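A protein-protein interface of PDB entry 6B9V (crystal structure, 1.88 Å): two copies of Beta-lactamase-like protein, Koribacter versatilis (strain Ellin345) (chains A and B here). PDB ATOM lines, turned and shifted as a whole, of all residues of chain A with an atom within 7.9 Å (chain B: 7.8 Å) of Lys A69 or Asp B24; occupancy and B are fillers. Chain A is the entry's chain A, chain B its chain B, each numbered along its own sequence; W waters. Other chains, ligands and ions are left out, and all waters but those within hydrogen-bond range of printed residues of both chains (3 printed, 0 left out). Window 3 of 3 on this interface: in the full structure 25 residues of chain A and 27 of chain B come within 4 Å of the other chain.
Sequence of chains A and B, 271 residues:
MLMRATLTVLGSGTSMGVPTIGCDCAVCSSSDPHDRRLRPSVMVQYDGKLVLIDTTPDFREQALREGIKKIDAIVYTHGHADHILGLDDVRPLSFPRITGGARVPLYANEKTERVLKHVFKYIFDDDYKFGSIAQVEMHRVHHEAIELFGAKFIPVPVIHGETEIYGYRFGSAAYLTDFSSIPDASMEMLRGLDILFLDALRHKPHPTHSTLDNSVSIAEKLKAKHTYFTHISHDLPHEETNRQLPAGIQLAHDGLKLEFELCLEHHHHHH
The side-chain carboxylate of Asp B24 lies within salt-bridge range of the side-chain amino group of Lys A69, 2.8 Å away.
No position is printed for both chains.
Of the 9 pairs that touch across the chains among the printed residues, none has its exchanged pair printed and touching as well.
The backbone carbonyl oxygen (O) of Ala A63 is in hydrogen-bond range of the backbone NH (N) of Ile A68.
The backbone NH (N) of Thr B20 lies close to the side-chain sulfur (SG) of Cys B28, 3.3 Å away.
Of the printed residues of chain B, Ile A68 touches Gly B22.
Of the printed residues of chain A, Thr B20 touches Pro A92 (3.7 Å).
Printed residues of chain A within 4 Å of Gly B22: Ile A68 (3.96 Å), Lys A69 (3.8 Å) and Leu A93 (3.8 Å).
Of the printed residues of chain A, Cys B23 touches Lys A69.
Of chain A, only Lys A69 (2.8 Å) comes within 4 Å of Asp B24.
The nearest residue of chain B that does not touch Lys A69 is Ile B21 (6.0 Å).
The nearest printed residue of chain A that does not touch Gly B22 is Ile A98 (4.3 Å).
Of the 11 printed residues of chain B, 5 touch a printed residue of chain A.
Hydrophobic or aromatic side chains of chain B within 4 Å of the printed part of chain A: Ile B21.
Of the 17 printed residues of chain A, 5 touch a printed residue of chain B.
Among the printed residues, Asp or Glu carboxylates within 4 Å of a Lys or Arg side-chain nitrogen of the other chain: Lys A69 with Asp B24 (2.8 Å).
Water W3 bridges the backbone carbonyl oxygen of Ile B21 (2.7 Å) and the backbone carbonyl oxygen of Pro A92 (3.3 Å).
Water W2 bridges the backbone carbonyl oxygen (O) of Ile A68 (2.7 Å) and the backbone NH (N) of Gly B22 (3.0 Å).
Water W1 lies within hydrogen-bond range of NZ of Lys A69 (2.7 Å) and N of Gly B22 (3.2 Å).
Among the printed residues, merely in contact across the chains: Lys A69 with Cys B23, Leu A93 with Ile B21, Leu A64 with Ile B21, Pro A92 with Thr B20, Lys A69 with Gly B22, Leu A93 with Gly B22, Ile A68 with Gly B22 and Pro A92 with Ile B21.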
ATOM      1  N   GLN A  45      12.136 -25.502  21.418  1.00  0.00           N
ATOM      2  CA  GLN A  45      13.583 -25.635  21.297  1.00  0.00           C
ATOM      3  C   GLN A  45      14.091 -26.801  22.116  1.00  0.00           C
ATOM      4  O   GLN A  45      13.714 -26.965  23.280  1.00  0.00           O
ATOM      5  CB  GLN A  45      14.285 -24.348  21.733  1.00  0.00           C
ATOM      6  CG  GLN A  45      14.114 -23.238  20.744  1.00  0.00           C
ATOM      7  CD  GLN A  45      14.512 -21.901  21.305  1.00  0.00           C
ATOM      8  OE1 GLN A  45      13.983 -21.470  22.321  1.00  0.00           O
ATOM      9  NE2 GLN A  45      15.465 -21.243  20.653  1.00  0.00           N
ATOM     10  N   LEU A  50      15.240 -26.043  16.633  1.00  0.00           N
ATOM     11  CA  LEU A  50      14.087 -25.158  16.763  1.00  0.00           C
ATOM     12  C   LEU A  50      12.969 -25.608  15.818  1.00  0.00           C
ATOM     13  O   LEU A  50      13.155 -25.665  14.599  1.00  0.00           O
ATOM     14  CB  LEU A  50      14.494 -23.706  16.471  1.00  0.00           C
ATOM     15  CG  LEU A  50      13.540 -22.539  16.781  1.00  0.00           C
ATOM     16  CD1 LEU A  50      14.316 -21.222  16.772  1.00  0.00           C
ATOM     17  CD2 LEU A  50      12.383 -22.462  15.789  1.00  0.00           C
ATOM     18  N   ALA A  63      10.160 -13.519  14.868  1.00  0.00           N
ATOM     19  CA  ALA A  63      11.517 -14.031  14.733  1.00  0.00           C
ATOM     20  C   ALA A  63      12.555 -13.011  15.210  1.00  0.00           C
ATOM     21  O   ALA A  63      13.497 -13.359  15.913  1.00  0.00           O
ATOM     22  CB  ALA A  63      11.795 -14.429  13.272  1.00  0.00           C
ATOM     23  N   LEU A  64      12.385 -11.753  14.826  1.00  0.00           N
ATOM     24  CA  LEU A  64      13.338 -10.719  15.230  1.00  0.00           C
ATOM     25  C   LEU A  64      13.322 -10.548  16.734  1.00  0.00           C
ATOM     26  O   LEU A  64      14.366 -10.458  17.371  1.00  0.00           O
ATOM     27  CB  LEU A  64      13.015  -9.382  14.542  1.00  0.00           C
ATOM     28  CG  LEU A  64      13.276  -9.338  13.042  1.00  0.00           C
ATOM     29  CD1 LEU A  64      12.731  -8.030  12.471  1.00  0.00           C
ATOM     30  CD2 LEU A  64      14.797  -9.471  12.772  1.00  0.00           C
ATOM     31  N   GLU A  66      12.615 -12.718  18.978  1.00  0.00           N
ATOM     32  CA  GLU A  66      13.231 -13.816  19.709  1.00  0.00           C
ATOM     33  C   GLU A  66      14.633 -14.195  19.231  1.00  0.00           C
ATOM     34  O   GLU A  66      15.213 -15.177  19.714  1.00  0.00           O
ATOM     35  CB  GLU A  66      12.323 -15.038  19.644  1.00  0.00           C
ATOM     36  CG  GLU A  66      11.018 -14.842  20.391  1.00  0.00           C
ATOM     37  CD  GLU A  66      11.208 -14.907  21.895  1.00  0.00           C
ATOM     38  OE1 GLU A  66      10.287 -14.502  22.641  1.00  0.00           O
ATOM     39  OE2 GLU A  66      12.285 -15.370  22.332  1.00  0.00           O
ATOM     40  N   GLY A  67      15.175 -13.427  18.292  1.00  0.00           N
ATOM     41  CA  GLY A  67      16.518 -13.665  17.780  1.00  0.00           C
ATOM     42  C   GLY A  67      16.686 -14.981  17.039  1.00  0.00           C
ATOM     43  O   GLY A  67      17.756 -15.589  17.092  1.00  0.00           O
ATOM     44  N   ILE A  68      15.639 -15.427  16.345  1.00  0.00           N
ATOM     45  CA  ILE A  68      15.720 -16.664  15.565  1.00  0.00           C
ATOM     46  C   ILE A  68      16.703 -16.525  14.400  1.00  0.00           C
ATOM     47  O   ILE A  68      16.588 -15.611  13.583  1.00  0.00           O
ATOM     48  CB  ILE A  68      14.348 -17.078  15.015  1.00  0.00           C
ATOM     49  CG1 ILE A  68      13.390 -17.407  16.171  1.00  0.00           C
ATOM     50  CG2 ILE A  68      14.487 -18.272  14.052  1.00  0.00           C
ATOM     51  CD1 ILE A  68      11.963 -17.682  15.715  1.00  0.00           C
ATOM     52  N   LYS A  69      17.664 -17.442  14.330  1.00  0.00           N
ATOM     53  CA  LYS A  69      18.701 -17.399  13.301  1.00  0.00           C
ATOM     54  C   LYS A  69      18.608 -18.607  12.373  1.00  0.00           C
ATOM     55  O   LYS A  69      19.252 -18.650  11.331  1.00  0.00           O
ATOM     56  CB  LYS A  69      20.093 -17.351  13.943  1.00  0.00           C
ATOM     57  CG  LYS A  69      20.339 -16.157  14.859  1.00  0.00           C
ATOM     58  CD  LYS A  69      20.627 -14.889  14.061  1.00  0.00           C
ATOM     59  CE  LYS A  69      20.890 -13.695  14.972  1.00  0.00           C
ATOM     60  NZ  LYS A  69      21.103 -12.438  14.196  1.00  0.00           N
ATOM     61  N   LYS A  70      17.822 -19.599  12.773  1.00  0.00           N
ATOM     62  CA  LYS A  70      17.694 -20.843  12.024  1.00  0.00           C
ATOM     63  C   LYS A  70      16.421 -21.581  12.438  1.00  0.00           C
ATOM     64  O   LYS A  70      16.088 -21.640  13.623  1.00  0.00           O
ATOM     65  CB  LYS A  70      18.922 -21.736  12.250  1.00  0.00           C
ATOM     66  CG  LYS A  70      18.878 -23.062  11.508  1.00  0.00           C
ATOM     67  CD  LYS A  70      20.204 -23.807  11.603  1.00  0.00           C
ATOM     68  CE  LYS A  70      20.138 -25.148  10.874  1.00  0.00           C
ATOM     69  NZ  LYS A  70      21.473 -25.809  10.862  1.00  0.00           N
ATOM     70  N   ILE A  71      15.718 -22.136  11.461  1.00  0.00           N
ATOM     71  CA  ILE A  71      14.543 -22.960  11.729  1.00  0.00           C
ATOM     72  C   ILE A  71      14.799 -24.373  11.234  1.00  0.00           C
ATOM     73  O   ILE A  71      15.112 -24.569  10.065  1.00  0.00           O
ATOM     74  CB  ILE A  71      13.283 -22.416  11.041  1.00  0.00           C
ATOM     75  CG1 ILE A  71      12.967 -20.995  11.517  1.00  0.00           C
ATOM     76  CG2 ILE A  71      12.099 -23.364  11.296  1.00  0.00           C
ATOM     77  CD1 ILE A  71      11.954 -20.278  10.622  1.00  0.00           C
ATOM     78  N   ASP A  72      14.668 -25.365  12.111  1.00  0.00           N
ATOM     79  CA  ASP A  72      14.963 -26.729  11.690  1.00  0.00           C
ATOM     80  C   ASP A  72      13.774 -27.448  11.072  1.00  0.00           C
ATOM     81  O   ASP A  72      13.946 -28.335  10.238  1.00  0.00           O
ATOM     82  CB  ASP A  72      15.528 -27.516  12.870  1.00  0.00           C
ATOM     83  CG  ASP A  72      16.853 -26.933  13.348  1.00  0.00           C
ATOM     84  OD1 ASP A  72      17.891 -27.213  12.703  1.00  0.00           O
ATOM     85  OD2 ASP A  72      16.846 -26.154  14.330  1.00  0.00           O
ATOM     86  N   PRO A  92      14.438 -15.621   4.008  1.00  0.00           N
ATOM     87  CA  PRO A  92      15.870 -15.380   4.261  1.00  0.00           C
ATOM     88  C   PRO A  92      16.537 -16.401   5.195  1.00  0.00           C
ATOM     89  O   PRO A  92      17.766 -16.426   5.285  1.00  0.00           O
ATOM     90  CB  PRO A  92      15.890 -13.987   4.915  1.00  0.00           C
ATOM     91  CG  PRO A  92      14.540 -13.397   4.640  1.00  0.00           C
ATOM     92  CD  PRO A  92      13.603 -14.559   4.594  1.00  0.00           C
ATOM     93  N   LEU A  93      15.754 -17.219   5.893  1.00  0.00           N
ATOM     94  CA  LEU A  93      16.340 -18.276   6.713  1.00  0.00           C
ATOM     95  C   LEU A  93      16.504 -19.582   5.938  1.00  0.00           C
ATOM     96  O   LEU A  93      17.052 -20.557   6.465  1.00  0.00           O
ATOM     97  CB  LEU A  93      15.484 -18.537   7.964  1.00  0.00           C
ATOM     98  CG  LEU A  93      15.423 -17.370   8.954  1.00  0.00           C
ATOM     99  CD1 LEU A  93      14.530 -17.721  10.143  1.00  0.00           C
ATOM    100  CD2 LEU A  93      16.826 -16.950   9.411  1.00  0.00           C
ATOM    101  N   SER A  94      16.028 -19.610   4.696  1.00  0.00           N
ATOM    102  CA  SER A  94      15.995 -20.861   3.930  1.00  0.00           C
ATOM    103  C   SER A  94      17.162 -21.028   2.959  1.00  0.00           C
ATOM    104  O   SER A  94      17.244 -22.032   2.243  1.00  0.00           O
ATOM    105  CB  SER A  94      14.688 -20.965   3.143  1.00  0.00           C
ATOM    106  OG  SER A  94      14.642 -19.980   2.123  1.00  0.00           O
ATOM    107  N   ARG A  97      23.414 -20.883   2.970  1.00  0.00           N
ATOM    108  CA  ARG A  97      24.293 -20.195   3.908  1.00  0.00           C
ATOM    109  C   ARG A  97      23.887 -20.469   5.343  1.00  0.00           C
ATOM    110  O   ARG A  97      24.714 -20.834   6.176  1.00  0.00           O
ATOM    111  CB  ARG A  97      24.262 -18.685   3.665  1.00  0.00           C
ATOM    112  CG  ARG A  97      24.206 -18.266   2.205  1.00  0.00           C
ATOM    113  CD  ARG A  97      23.255 -17.087   2.028  1.00  0.00           C
ATOM    114  NE  ARG A  97      23.269 -16.192   3.181  1.00  0.00           N
ATOM    115  CZ  ARG A  97      22.518 -15.101   3.288  1.00  0.00           C
ATOM    116  NH1 ARG A  97      21.694 -14.763   2.306  1.00  0.00           N
ATOM    117  NH2 ARG A  97      22.595 -14.346   4.377  1.00  0.00           N
ATOM    118  N   ILE A  98      22.597 -20.288   5.616  1.00  0.00           N
ATOM    119  CA  ILE A  98      22.054 -20.425   6.961  1.00  0.00           C
ATOM    120  C   ILE A  98      21.679 -21.867   7.290  1.00  0.00           C
ATOM    121  O   ILE A  98      21.946 -22.348   8.393  1.00  0.00           O
ATOM    122  CB  ILE A  98      20.808 -19.523   7.154  1.00  0.00           C
ATOM    123  CG1 ILE A  98      21.233 -18.058   7.277  1.00  0.00           C
ATOM    124  CG2 ILE A  98      20.001 -19.945   8.382  1.00  0.00           C
ATOM    125  CD1 ILE A  98      20.125 -17.148   7.727  1.00  0.00           C
ATOM    126  N   THR A  99      21.064 -22.555   6.338  1.00  0.00           N
ATOM    127  CA  THR A  99      20.528 -23.881   6.613  1.00  0.00           C
ATOM    128  C   THR A  99      21.641 -24.899   6.782  1.00  0.00           C
ATOM    129  O   THR A  99      21.555 -25.798   7.617  1.00  0.00           O
ATOM    130  CB  THR A  99      19.590 -24.367   5.496  1.00  0.00           C
ATOM    131  OG1 THR A  99      20.306 -24.396   4.255  1.00  0.00           O
ATOM    132  CG2 THR A  99      18.361 -23.459   5.370  1.00  0.00           C
ATOM    133  N   THR B  20      17.012  -7.699   8.347  1.00  0.00           N
ATOM    134  CA  THR B  20      16.630  -8.956   7.695  1.00  0.00           C
ATOM    135  C   THR B  20      16.819 -10.047   8.729  1.00  0.00           C
ATOM    136  O   THR B  20      17.860 -10.103   9.380  1.00  0.00           O
ATOM    137  CB  THR B  20      17.497  -9.265   6.447  1.00  0.00           C
ATOM    138  OG1 THR B  20      17.168  -8.359   5.391  1.00  0.00           O
ATOM    139  CG2 THR B  20      17.262 -10.689   5.961  1.00  0.00           C
ATOM    140  N   ILE B  21      15.821 -10.902   8.904  1.00  0.00           N
ATOM    141  CA  ILE B  21      15.930 -11.937   9.918  1.00  0.00           C
ATOM    142  C   ILE B  21      17.155 -12.804   9.683  1.00  0.00           C
ATOM    143  O   ILE B  21      17.495 -13.124   8.546  1.00  0.00           O
ATOM    144  CB  ILE B  21      14.680 -12.818   9.967  1.00  0.00           C
ATOM    145  CG1 ILE B  21      14.415 -13.466   8.612  1.00  0.00           C
ATOM    146  CG2 ILE B  21      13.479 -11.994  10.401  1.00  0.00           C
ATOM    147  CD1 ILE B  21      13.262 -14.452   8.681  1.00  0.00           C
ATOM    148  N   GLY B  22      17.847 -13.122  10.772  1.00  0.00           N
ATOM    149  CA  GLY B  22      18.964 -14.037  10.723  1.00  0.00           C
ATOM    150  C   GLY B  22      20.282 -13.359  10.389  1.00  0.00           C
ATOM    151  O   GLY B  22      21.317 -13.998  10.475  1.00  0.00           O
ATOM    152  N   CYS B  23      20.243 -12.083   9.999  1.00  0.00           N
ATOM    153  CA  CYS B  23      21.455 -11.369   9.569  1.00  0.00           C
ATOM    154  C   CYS B  23      22.196 -10.729  10.728  1.00  0.00           C
ATOM    155  O   CYS B  23      21.585 -10.076  11.575  1.00  0.00           O
ATOM    156  CB  CYS B  23      21.118 -10.280   8.540  1.00  0.00           C
ATOM    157  SG  CYS B  23      22.619  -9.482   7.873  1.00  0.00           S
ATOM    158  N   ASP B  24      23.519 -10.870  10.729  1.00  0.00           N
ATOM    159  CA  ASP B  24      24.338 -10.322  11.796  1.00  0.00           C
ATOM    160  C   ASP B  24      25.052  -9.020  11.438  1.00  0.00           C
ATOM    161  O   ASP B  24      25.864  -8.551  12.228  1.00  0.00           O
ATOM    162  CB  ASP B  24      25.394 -11.342  12.226  1.00  0.00           C
ATOM    163  CG  ASP B  24      24.790 -12.576  12.853  1.00  0.00           C
ATOM    164  OD1 ASP B  24      23.790 -12.444  13.594  1.00  0.00           O
ATOM    165  OD2 ASP B  24      25.314 -13.677  12.594  1.00  0.00           O
ATOM    166  N   CYS B  25      24.777  -8.452  10.264  1.00  0.00           N
ATOM    167  CA  CYS B  25      25.524  -7.260   9.831  1.00  0.00           C
ATOM    168  C   CYS B  25      25.241  -6.079  10.767  1.00  0.00           C
ATOM    169  O   CYS B  25      24.289  -6.104  11.553  1.00  0.00           O
ATOM    170  CB  CYS B  25      25.193  -6.895   8.372  1.00  0.00           C
ATOM    171  SG  CYS B  25      23.738  -5.828   8.128  1.00  0.00           S
ATOM    172  N   ALA B  26      26.066  -5.042  10.684  1.00  0.00           N
ATOM    173  CA  ALA B  26      25.973  -3.922  11.621  1.00  0.00           C
ATOM    174  C   ALA B  26      24.643  -3.187  11.512  1.00  0.00           C
ATOM    175  O   ALA B  26      24.035  -2.824  12.519  1.00  0.00           O
ATOM    176  CB  ALA B  26      27.145  -2.947  11.396  1.00  0.00           C
ATOM    177  N   VAL B  27      24.179  -2.975  10.288  1.00  0.00           N
ATOM    178  CA  VAL B  27      22.929  -2.256  10.083  1.00  0.00           C
ATOM    179  C   VAL B  27      21.760  -3.055  10.664  1.00  0.00           C
ATOM    180  O   VAL B  27      20.837  -2.489  11.234  1.00  0.00           O
ATOM    181  CB  VAL B  27      22.677  -1.956   8.584  1.00  0.00           C
ATOM    182  CG1 VAL B  27      21.251  -1.425   8.358  1.00  0.00           C
ATOM    183  CG2 VAL B  27      23.699  -0.946   8.076  1.00  0.00           C
ATOM    184  N   CYS B  28      21.826  -4.378  10.571  1.00  0.00           N
ATOM    185  CA  CYS B  28      20.739  -5.191  11.102  1.00  0.00           C
ATOM    186  C   CYS B  28      20.762  -5.217  12.633  1.00  0.00           C
ATOM    187  O   CYS B  28      19.787  -5.622  13.259  1.00  0.00           O
ATOM    188  CB  CYS B  28      20.794  -6.604  10.514  1.00  0.00           C
ATOM    189  SG  CYS B  28      20.085  -6.676   8.831  1.00  0.00           S
ATOM    190  N   SER B  29      21.858  -4.744  13.226  1.00  0.00           N
ATOM    191  CA  SER B  29      21.964  -4.604  14.679  1.00  0.00           C
ATOM    192  C   SER B  29      22.006  -3.142  15.130  1.00  0.00           C
ATOM    193  O   SER B  29      22.426  -2.858  16.241  1.00  0.00           O
ATOM    194  CB  SER B  29      23.222  -5.313  15.197  1.00  0.00           C
ATOM    195  OG  SER B  29      23.107  -6.716  15.070  1.00  0.00           O
ATOM    196  N   HIS B 234      19.513  -3.379   4.016  1.00  0.00           N
ATOM    197  CA  HIS B 234      20.516  -3.317   5.085  1.00  0.00           C
ATOM    198  C   HIS B 234      21.920  -2.888   4.603  1.00  0.00           C
ATOM    199  O   HIS B 234      22.811  -2.625   5.424  1.00  0.00           O
ATOM    200  CB  HIS B 234      20.555  -4.684   5.812  1.00  0.00           C
ATOM    201  CG  HIS B 234      20.977  -5.834   4.940  1.00  0.00           C
ATOM    202  ND1 HIS B 234      21.402  -7.040   5.448  1.00  0.00           N
ATOM    203  CD2 HIS B 234      21.132  -5.919   3.594  1.00  0.00           C
ATOM    204  CE1 HIS B 234      21.741  -7.846   4.458  1.00  0.00           C
ATOM    205  NE2 HIS B 234      21.596  -7.187   3.319  1.00  0.00           N
HETATM  206  O   HOH W   1      18.489 -11.882  13.686  1.00  0.00           O
HETATM  207  O   HOH W   2      16.332 -12.928  13.390  1.00  0.00           O
HETATM  208  O   HOH W   3      19.342 -13.899   6.756  1.00  0.00           O
